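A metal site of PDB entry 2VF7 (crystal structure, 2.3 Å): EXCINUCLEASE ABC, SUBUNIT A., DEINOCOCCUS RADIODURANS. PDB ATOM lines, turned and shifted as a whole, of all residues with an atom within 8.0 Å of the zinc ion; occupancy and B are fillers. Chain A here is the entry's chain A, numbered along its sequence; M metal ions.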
ATOM      1  N   ARG A 640     -22.885 -16.089  22.748  1.00  0.00           N
ATOM      2  CA  ARG A 640     -21.894 -16.762  23.592  1.00  0.00           C
ATOM      3  C   ARG A 640     -22.073 -16.452  25.076  1.00  0.00           C
ATOM      4  O   ARG A 640     -22.743 -15.488  25.474  1.00  0.00           O
ATOM      5  CB  ARG A 640     -20.480 -16.368  23.171  1.00  0.00           C
ATOM      6  CG  ARG A 640     -20.205 -14.879  23.178  1.00  0.00           C
ATOM      7  CD  ARG A 640     -18.707 -14.589  22.994  1.00  0.00           C
ATOM      8  NE  ARG A 640     -18.391 -13.212  23.368  1.00  0.00           N
ATOM      9  CZ  ARG A 640     -17.261 -12.580  23.058  1.00  0.00           C
ATOM     10  NH1 ARG A 640     -16.338 -13.185  22.339  1.00  0.00           N
ATOM     11  NH2 ARG A 640     -17.069 -11.343  23.441  1.00  0.00           N
ATOM     12  N   CYS A 641     -21.443 -17.275  25.903  1.00  0.00           N
ATOM     13  CA  CYS A 641     -21.344 -16.972  27.320  1.00  0.00           C
ATOM     14  C   CYS A 641     -20.375 -15.820  27.462  1.00  0.00           C
ATOM     15  O   CYS A 641     -19.225 -15.916  27.030  1.00  0.00           O
ATOM     16  CB  CYS A 641     -20.865 -18.198  28.086  1.00  0.00           C
ATOM     17  SG  CYS A 641     -20.535 -17.857  29.797  1.00  0.00           S
ATOM     18  N   GLU A 642     -20.832 -14.732  28.041  1.00  0.00           N
ATOM     19  CA  GLU A 642     -19.991 -13.556  28.153  1.00  0.00           C
ATOM     20  C   GLU A 642     -19.155 -13.546  29.427  1.00  0.00           C
ATOM     21  O   GLU A 642     -18.294 -12.682  29.589  1.00  0.00           O
ATOM     22  CB  GLU A 642     -20.814 -12.260  28.048  1.00  0.00           C
ATOM     23  CG  GLU A 642     -20.049 -11.147  27.338  1.00  0.00           C
ATOM     24  CD  GLU A 642     -19.711 -11.530  25.899  1.00  0.00           C
ATOM     25  OE1 GLU A 642     -20.459 -12.343  25.304  1.00  0.00           O
ATOM     26  OE2 GLU A 642     -18.694 -11.048  25.363  1.00  0.00           O
ATOM     27  N   HIS A 643     -19.405 -14.504  30.318  1.00  0.00           N
ATOM     28  CA  HIS A 643     -18.616 -14.625  31.558  1.00  0.00           C
ATOM     29  C   HIS A 643     -17.173 -15.062  31.237  1.00  0.00           C
ATOM     30  O   HIS A 643     -16.222 -14.600  31.868  1.00  0.00           O
ATOM     31  CB  HIS A 643     -19.297 -15.601  32.524  1.00  0.00           C
ATOM     32  CG  HIS A 643     -18.575 -15.781  33.834  1.00  0.00           C
ATOM     33  ND1 HIS A 643     -18.913 -15.086  34.969  1.00  0.00           N
ATOM     34  CD2 HIS A 643     -17.544 -16.597  34.178  1.00  0.00           C
ATOM     35  CE1 HIS A 643     -18.125 -15.455  35.961  1.00  0.00           C
ATOM     36  NE2 HIS A 643     -17.279 -16.367  35.509  1.00  0.00           N
ATOM     37  N   CYS A 644     -17.038 -15.934  30.237  1.00  0.00           N
ATOM     38  CA  CYS A 644     -15.758 -16.439  29.754  1.00  0.00           C
ATOM     39  C   CYS A 644     -15.500 -15.939  28.338  1.00  0.00           C
ATOM     40  O   CYS A 644     -14.516 -16.328  27.740  1.00  0.00           O
ATOM     41  CB  CYS A 644     -15.766 -17.957  29.731  1.00  0.00           C
ATOM     42  SG  CYS A 644     -17.140 -18.559  28.740  1.00  0.00           S
ATOM     43  N   GLN A 645     -16.404 -15.107  27.830  1.00  0.00           N
ATOM     44  CA  GLN A 645     -16.300 -14.547  26.481  1.00  0.00           C
ATOM     45  C   GLN A 645     -16.231 -15.657  25.420  1.00  0.00           C
ATOM     46  O   GLN A 645     -15.545 -15.536  24.407  1.00  0.00           O
ATOM     47  CB  GLN A 645     -15.086 -13.622  26.384  1.00  0.00           C
ATOM     48  CG  GLN A 645     -15.269 -12.216  26.941  1.00  0.00           C
ATOM     49  CD  GLN A 645     -14.302 -11.211  26.308  1.00  0.00           C
ATOM     50  OE1 GLN A 645     -13.459 -11.571  25.468  1.00  0.00           O
ATOM     51  NE2 GLN A 645     -14.430  -9.942  26.691  1.00  0.00           N
ATOM     52  N   GLY A 646     -16.935 -16.762  25.669  1.00  0.00           N
ATOM     53  CA  GLY A 646     -16.989 -17.852  24.704  1.00  0.00           C
ATOM     54  C   GLY A 646     -15.786 -18.786  24.646  1.00  0.00           C
ATOM     55  O   GLY A 646     -15.711 -19.614  23.740  1.00  0.00           O
ATOM     56  N   GLU A 647     -14.864 -18.658  25.596  1.00  0.00           N
ATOM     57  CA  GLU A 647     -13.694 -19.545  25.663  1.00  0.00           C
ATOM     58  C   GLU A 647     -13.982 -20.875  26.370  1.00  0.00           C
ATOM     59  O   GLU A 647     -13.252 -21.837  26.203  1.00  0.00           O
ATOM     60  CB  GLU A 647     -12.505 -18.853  26.336  1.00  0.00           C
ATOM     61  CG  GLU A 647     -12.117 -17.571  25.650  1.00  0.00           C
ATOM     62  CD  GLU A 647     -10.748 -17.057  26.007  1.00  0.00           C
ATOM     63  OE1 GLU A 647     -10.116 -17.609  26.945  1.00  0.00           O
ATOM     64  OE2 GLU A 647     -10.304 -16.104  25.339  1.00  0.00           O
ATOM     65  N   GLY A 648     -15.059 -20.915  27.149  1.00  0.00           N
ATOM     66  CA  GLY A 648     -15.525 -22.125  27.812  1.00  0.00           C
ATOM     67  C   GLY A 648     -14.757 -22.428  29.071  1.00  0.00           C
ATOM     68  O   GLY A 648     -15.207 -23.204  29.909  1.00  0.00           O
ATOM     69  N   TRP A 649     -13.593 -21.791  29.192  1.00  0.00           N
ATOM     70  CA  TRP A 649     -12.613 -22.029  30.237  1.00  0.00           C
ATOM     71  C   TRP A 649     -12.107 -20.735  30.845  1.00  0.00           C
ATOM     72  O   TRP A 649     -12.060 -19.690  30.188  1.00  0.00           O
ATOM     73  CB  TRP A 649     -11.450 -22.857  29.686  1.00  0.00           C
ATOM     74  CG  TRP A 649     -11.615 -24.310  29.997  1.00  0.00           C
ATOM     75  CD1 TRP A 649     -11.242 -24.962  31.139  1.00  0.00           C
ATOM     76  CD2 TRP A 649     -12.229 -25.291  29.160  1.00  0.00           C
ATOM     77  NE1 TRP A 649     -11.552 -26.305  31.063  1.00  0.00           N
ATOM     78  CE2 TRP A 649     -12.171 -26.529  29.856  1.00  0.00           C
ATOM     79  CE3 TRP A 649     -12.807 -25.253  27.901  1.00  0.00           C
ATOM     80  CZ2 TRP A 649     -12.678 -27.698  29.333  1.00  0.00           C
ATOM     81  CZ3 TRP A 649     -13.288 -26.415  27.363  1.00  0.00           C
ATOM     82  CH2 TRP A 649     -13.226 -27.622  28.080  1.00  0.00           C
ATOM     83  N   VAL A 650     -11.735 -20.794  32.118  1.00  0.00           N
ATOM     84  CA  VAL A 650     -11.286 -19.620  32.859  1.00  0.00           C
ATOM     85  C   VAL A 650      -9.934 -19.848  33.542  1.00  0.00           C
ATOM     86  O   VAL A 650      -9.673 -20.918  34.091  1.00  0.00           O
ATOM     87  CB  VAL A 650     -12.379 -19.147  33.880  1.00  0.00           C
ATOM     88  CG1 VAL A 650     -12.343 -19.973  35.188  1.00  0.00           C
ATOM     89  CG2 VAL A 650     -12.228 -17.663  34.166  1.00  0.00           C
ATOM     90  N   PRO A 663     -12.911 -25.137  34.054  1.00  0.00           N
ATOM     91  CA  PRO A 663     -14.100 -24.856  33.221  1.00  0.00           C
ATOM     92  C   PRO A 663     -14.856 -23.638  33.745  1.00  0.00           C
ATOM     93  O   PRO A 663     -14.872 -23.396  34.948  1.00  0.00           O
ATOM     94  CB  PRO A 663     -14.955 -26.122  33.357  1.00  0.00           C
ATOM     95  CG  PRO A 663     -14.046 -27.168  33.985  1.00  0.00           C
ATOM     96  CD  PRO A 663     -13.059 -26.398  34.810  1.00  0.00           C
ATOM     97  N   CYS A 664     -15.445 -22.851  32.846  1.00  0.00           N
ATOM     98  CA  CYS A 664     -16.207 -21.674  33.233  1.00  0.00           C
ATOM     99  C   CYS A 664     -17.329 -22.031  34.226  1.00  0.00           C
ATOM    100  O   CYS A 664     -18.075 -22.977  33.996  1.00  0.00           O
ATOM    101  CB  CYS A 664     -16.787 -21.025  31.980  1.00  0.00           C
ATOM    102  SG  CYS A 664     -17.853 -19.630  32.294  1.00  0.00           S
ATOM    103  N   PRO A 665     -17.428 -21.301  35.352  1.00  0.00           N
ATOM    104  CA  PRO A 665     -18.461 -21.567  36.353  1.00  0.00           C
ATOM    105  C   PRO A 665     -19.902 -21.351  35.883  1.00  0.00           C
ATOM    106  O   PRO A 665     -20.836 -21.803  36.535  1.00  0.00           O
ATOM    107  CB  PRO A 665     -18.119 -20.589  37.474  1.00  0.00           C
ATOM    108  CG  PRO A 665     -17.338 -19.518  36.811  1.00  0.00           C
ATOM    109  CD  PRO A 665     -16.539 -20.200  35.769  1.00  0.00           C
ATOM    110  N   VAL A 666     -20.086 -20.704  34.736  1.00  0.00           N
ATOM    111  CA  VAL A 666     -21.417 -20.331  34.253  1.00  0.00           C
ATOM    112  C   VAL A 666     -21.908 -21.195  33.083  1.00  0.00           C
ATOM    113  O   VAL A 666     -23.059 -21.580  33.041  1.00  0.00           O
ATOM    114  CB  VAL A 666     -21.449 -18.854  33.837  1.00  0.00           C
ATOM    115  CG1 VAL A 666     -22.840 -18.454  33.354  1.00  0.00           C
ATOM    116  CG2 VAL A 666     -21.027 -17.992  34.978  1.00  0.00           C
ATOM    117  N   CYS A 667     -21.053 -21.497  32.122  1.00  0.00           N
ATOM    118  CA  CYS A 667     -21.487 -22.358  31.034  1.00  0.00           C
ATOM    119  C   CYS A 667     -20.902 -23.751  31.193  1.00  0.00           C
ATOM    120  O   CYS A 667     -21.341 -24.687  30.533  1.00  0.00           O
ATOM    121  CB  CYS A 667     -21.148 -21.753  29.679  1.00  0.00           C
ATOM    122  SG  CYS A 667     -19.402 -21.660  29.347  1.00  0.00           S
ATOM    123  N   HIS A 668     -19.912 -23.883  32.075  1.00  0.00           N
ATOM    124  CA  HIS A 668     -19.283 -25.181  32.337  1.00  0.00           C
ATOM    125  C   HIS A 668     -18.575 -25.759  31.120  1.00  0.00           C
ATOM    126  O   HIS A 668     -18.361 -26.966  31.046  1.00  0.00           O
ATOM    127  CB  HIS A 668     -20.300 -26.201  32.861  1.00  0.00           C
ATOM    128  CG  HIS A 668     -20.970 -25.786  34.132  1.00  0.00           C
ATOM    129  ND1 HIS A 668     -22.220 -25.221  34.162  1.00  0.00           N
ATOM    130  CD2 HIS A 668     -20.551 -25.838  35.425  1.00  0.00           C
ATOM    131  CE1 HIS A 668     -22.556 -24.952  35.411  1.00  0.00           C
ATOM    132  NE2 HIS A 668     -21.554 -25.306  36.199  1.00  0.00           N
ATOM    133  N   GLY A 669     -18.194 -24.906  30.185  1.00  0.00           N
ATOM    134  CA  GLY A 669     -17.417 -25.339  29.035  1.00  0.00           C
ATOM    135  C   GLY A 669     -18.177 -25.455  27.738  1.00  0.00           C
ATOM    136  O   GLY A 669     -17.599 -25.832  26.739  1.00  0.00           O
ATOM    137  N   THR A 670     -19.476 -25.144  27.743  1.00  0.00           N
ATOM    138  CA  THR A 670     -20.274 -25.150  26.517  1.00  0.00           C
ATOM    139  C   THR A 670     -19.939 -23.979  25.617  1.00  0.00           C
ATOM    140  O   THR A 670     -19.935 -24.140  24.399  1.00  0.00           O
ATOM    141  CB  THR A 670     -21.807 -25.231  26.761  1.00  0.00           C
ATOM    142  OG1 THR A 670     -22.302 -23.981  27.285  1.00  0.00           O
ATOM    143  CG2 THR A 670     -22.158 -26.394  27.717  1.00  0.00           C
ATOM    144  N   ARG A 671     -19.604 -22.831  26.215  1.00  0.00           N
ATOM    145  CA  ARG A 671     -19.186 -21.577  25.523  1.00  0.00           C
ATOM    146  C   ARG A 671     -20.347 -20.645  25.118  1.00  0.00           C
ATOM    147  O   ARG A 671     -20.107 -19.558  24.570  1.00  0.00           O
ATOM    148  CB  ARG A 671     -18.377 -21.854  24.267  1.00  0.00           C
ATOM    149  CG  ARG A 671     -17.005 -22.407  24.399  1.00  0.00           C
ATOM    150  CD  ARG A 671     -16.381 -22.537  22.976  1.00  0.00           C
ATOM    151  NE  ARG A 671     -15.246 -23.458  22.911  1.00  0.00           N
ATOM    152  CZ  ARG A 671     -13.959 -23.085  22.817  1.00  0.00           C
ATOM    153  NH1 ARG A 671     -13.615 -21.812  22.767  1.00  0.00           N
ATOM    154  NH2 ARG A 671     -13.004 -24.019  22.751  1.00  0.00           N
ATOM    155  N   TYR A 672     -21.589 -21.061  25.382  1.00  0.00           N
ATOM    156  CA  TYR A 672     -22.773 -20.333  24.916  1.00  0.00           C
ATOM    157  C   TYR A 672     -23.751 -20.114  26.037  1.00  0.00           C
ATOM    158  O   TYR A 672     -23.761 -20.876  27.004  1.00  0.00           O
ATOM    159  CB  TYR A 672     -23.461 -21.074  23.769  1.00  0.00           C
ATOM    160  CG  TYR A 672     -22.618 -21.204  22.521  1.00  0.00           C
ATOM    161  CD1 TYR A 672     -22.649 -20.219  21.526  1.00  0.00           C
ATOM    162  CD2 TYR A 672     -21.747 -22.320  22.338  1.00  0.00           C
ATOM    163  CE1 TYR A 672     -21.851 -20.345  20.372  1.00  0.00           C
ATOM    164  CE2 TYR A 672     -20.949 -22.447  21.184  1.00  0.00           C
ATOM    165  CZ  TYR A 672     -21.010 -21.452  20.218  1.00  0.00           C
ATOM    166  OH  TYR A 672     -20.252 -21.568  19.076  1.00  0.00           O
ATOM    167  N   ASN A 673     -24.596 -19.083  25.914  1.00  0.00           N
ATOM    168  CA  ASN A 673     -25.693 -18.898  26.873  1.00  0.00           C
ATOM    169  C   ASN A 673     -26.753 -19.971  26.669  1.00  0.00           C
ATOM    170  O   ASN A 673     -26.662 -20.741  25.720  1.00  0.00           O
ATOM    171  CB  ASN A 673     -26.247 -17.449  26.916  1.00  0.00           C
ATOM    172  CG  ASN A 673     -26.882 -17.011  25.608  1.00  0.00           C
ATOM    173  OD1 ASN A 673     -27.490 -17.807  24.899  1.00  0.00           O
ATOM    174  ND2 ASN A 673     -26.769 -15.729  25.300  1.00  0.00           N
HETATM  175 ZN    ZN M   1     -18.773 -19.555  30.056  1.00  0.00          ZN
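SG of Cys 667 lies close to N of Arg 671. The backbone NH of Gly 669 lies close to the side-chain sulfur of Cys 667 (3.6 Å). The side-chain hydroxyl of Thr 670 sits close to the backbone carbonyl oxygen of Cys 667. The side-chain sulfur (SG) of Cys 644 sits close to the backbone NH (N) of Gly 648, 3.5 Å away. The backbone NH (N) of Gly 646 lies close to the side-chain sulfur (SG) of Cys 644, at 3.6 Å. SG of Cys 664 lies close to N of Val 666, at 3.5 Å. The backbone NH of His 643 lies close to the side-chain sulfur of Cys 641 (3.6 Å). The backbone NH (N) of Cys 641 lies within hydrogen-bond range of the backbone carbonyl oxygen (O) of Arg 671, at 3.0 Å.
Four residues have an atom within 4 Å of the zinc ion: Cys 641, Cys 644, Cys 664 and Cys 667. The nearest printed residue that does not touch the zinc ion is Val 666 (4.7 Å).
The zinc ion is bound by SG of Cys 667, SG of Cys 644, SG of Cys 664 and SG of Cys 641.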
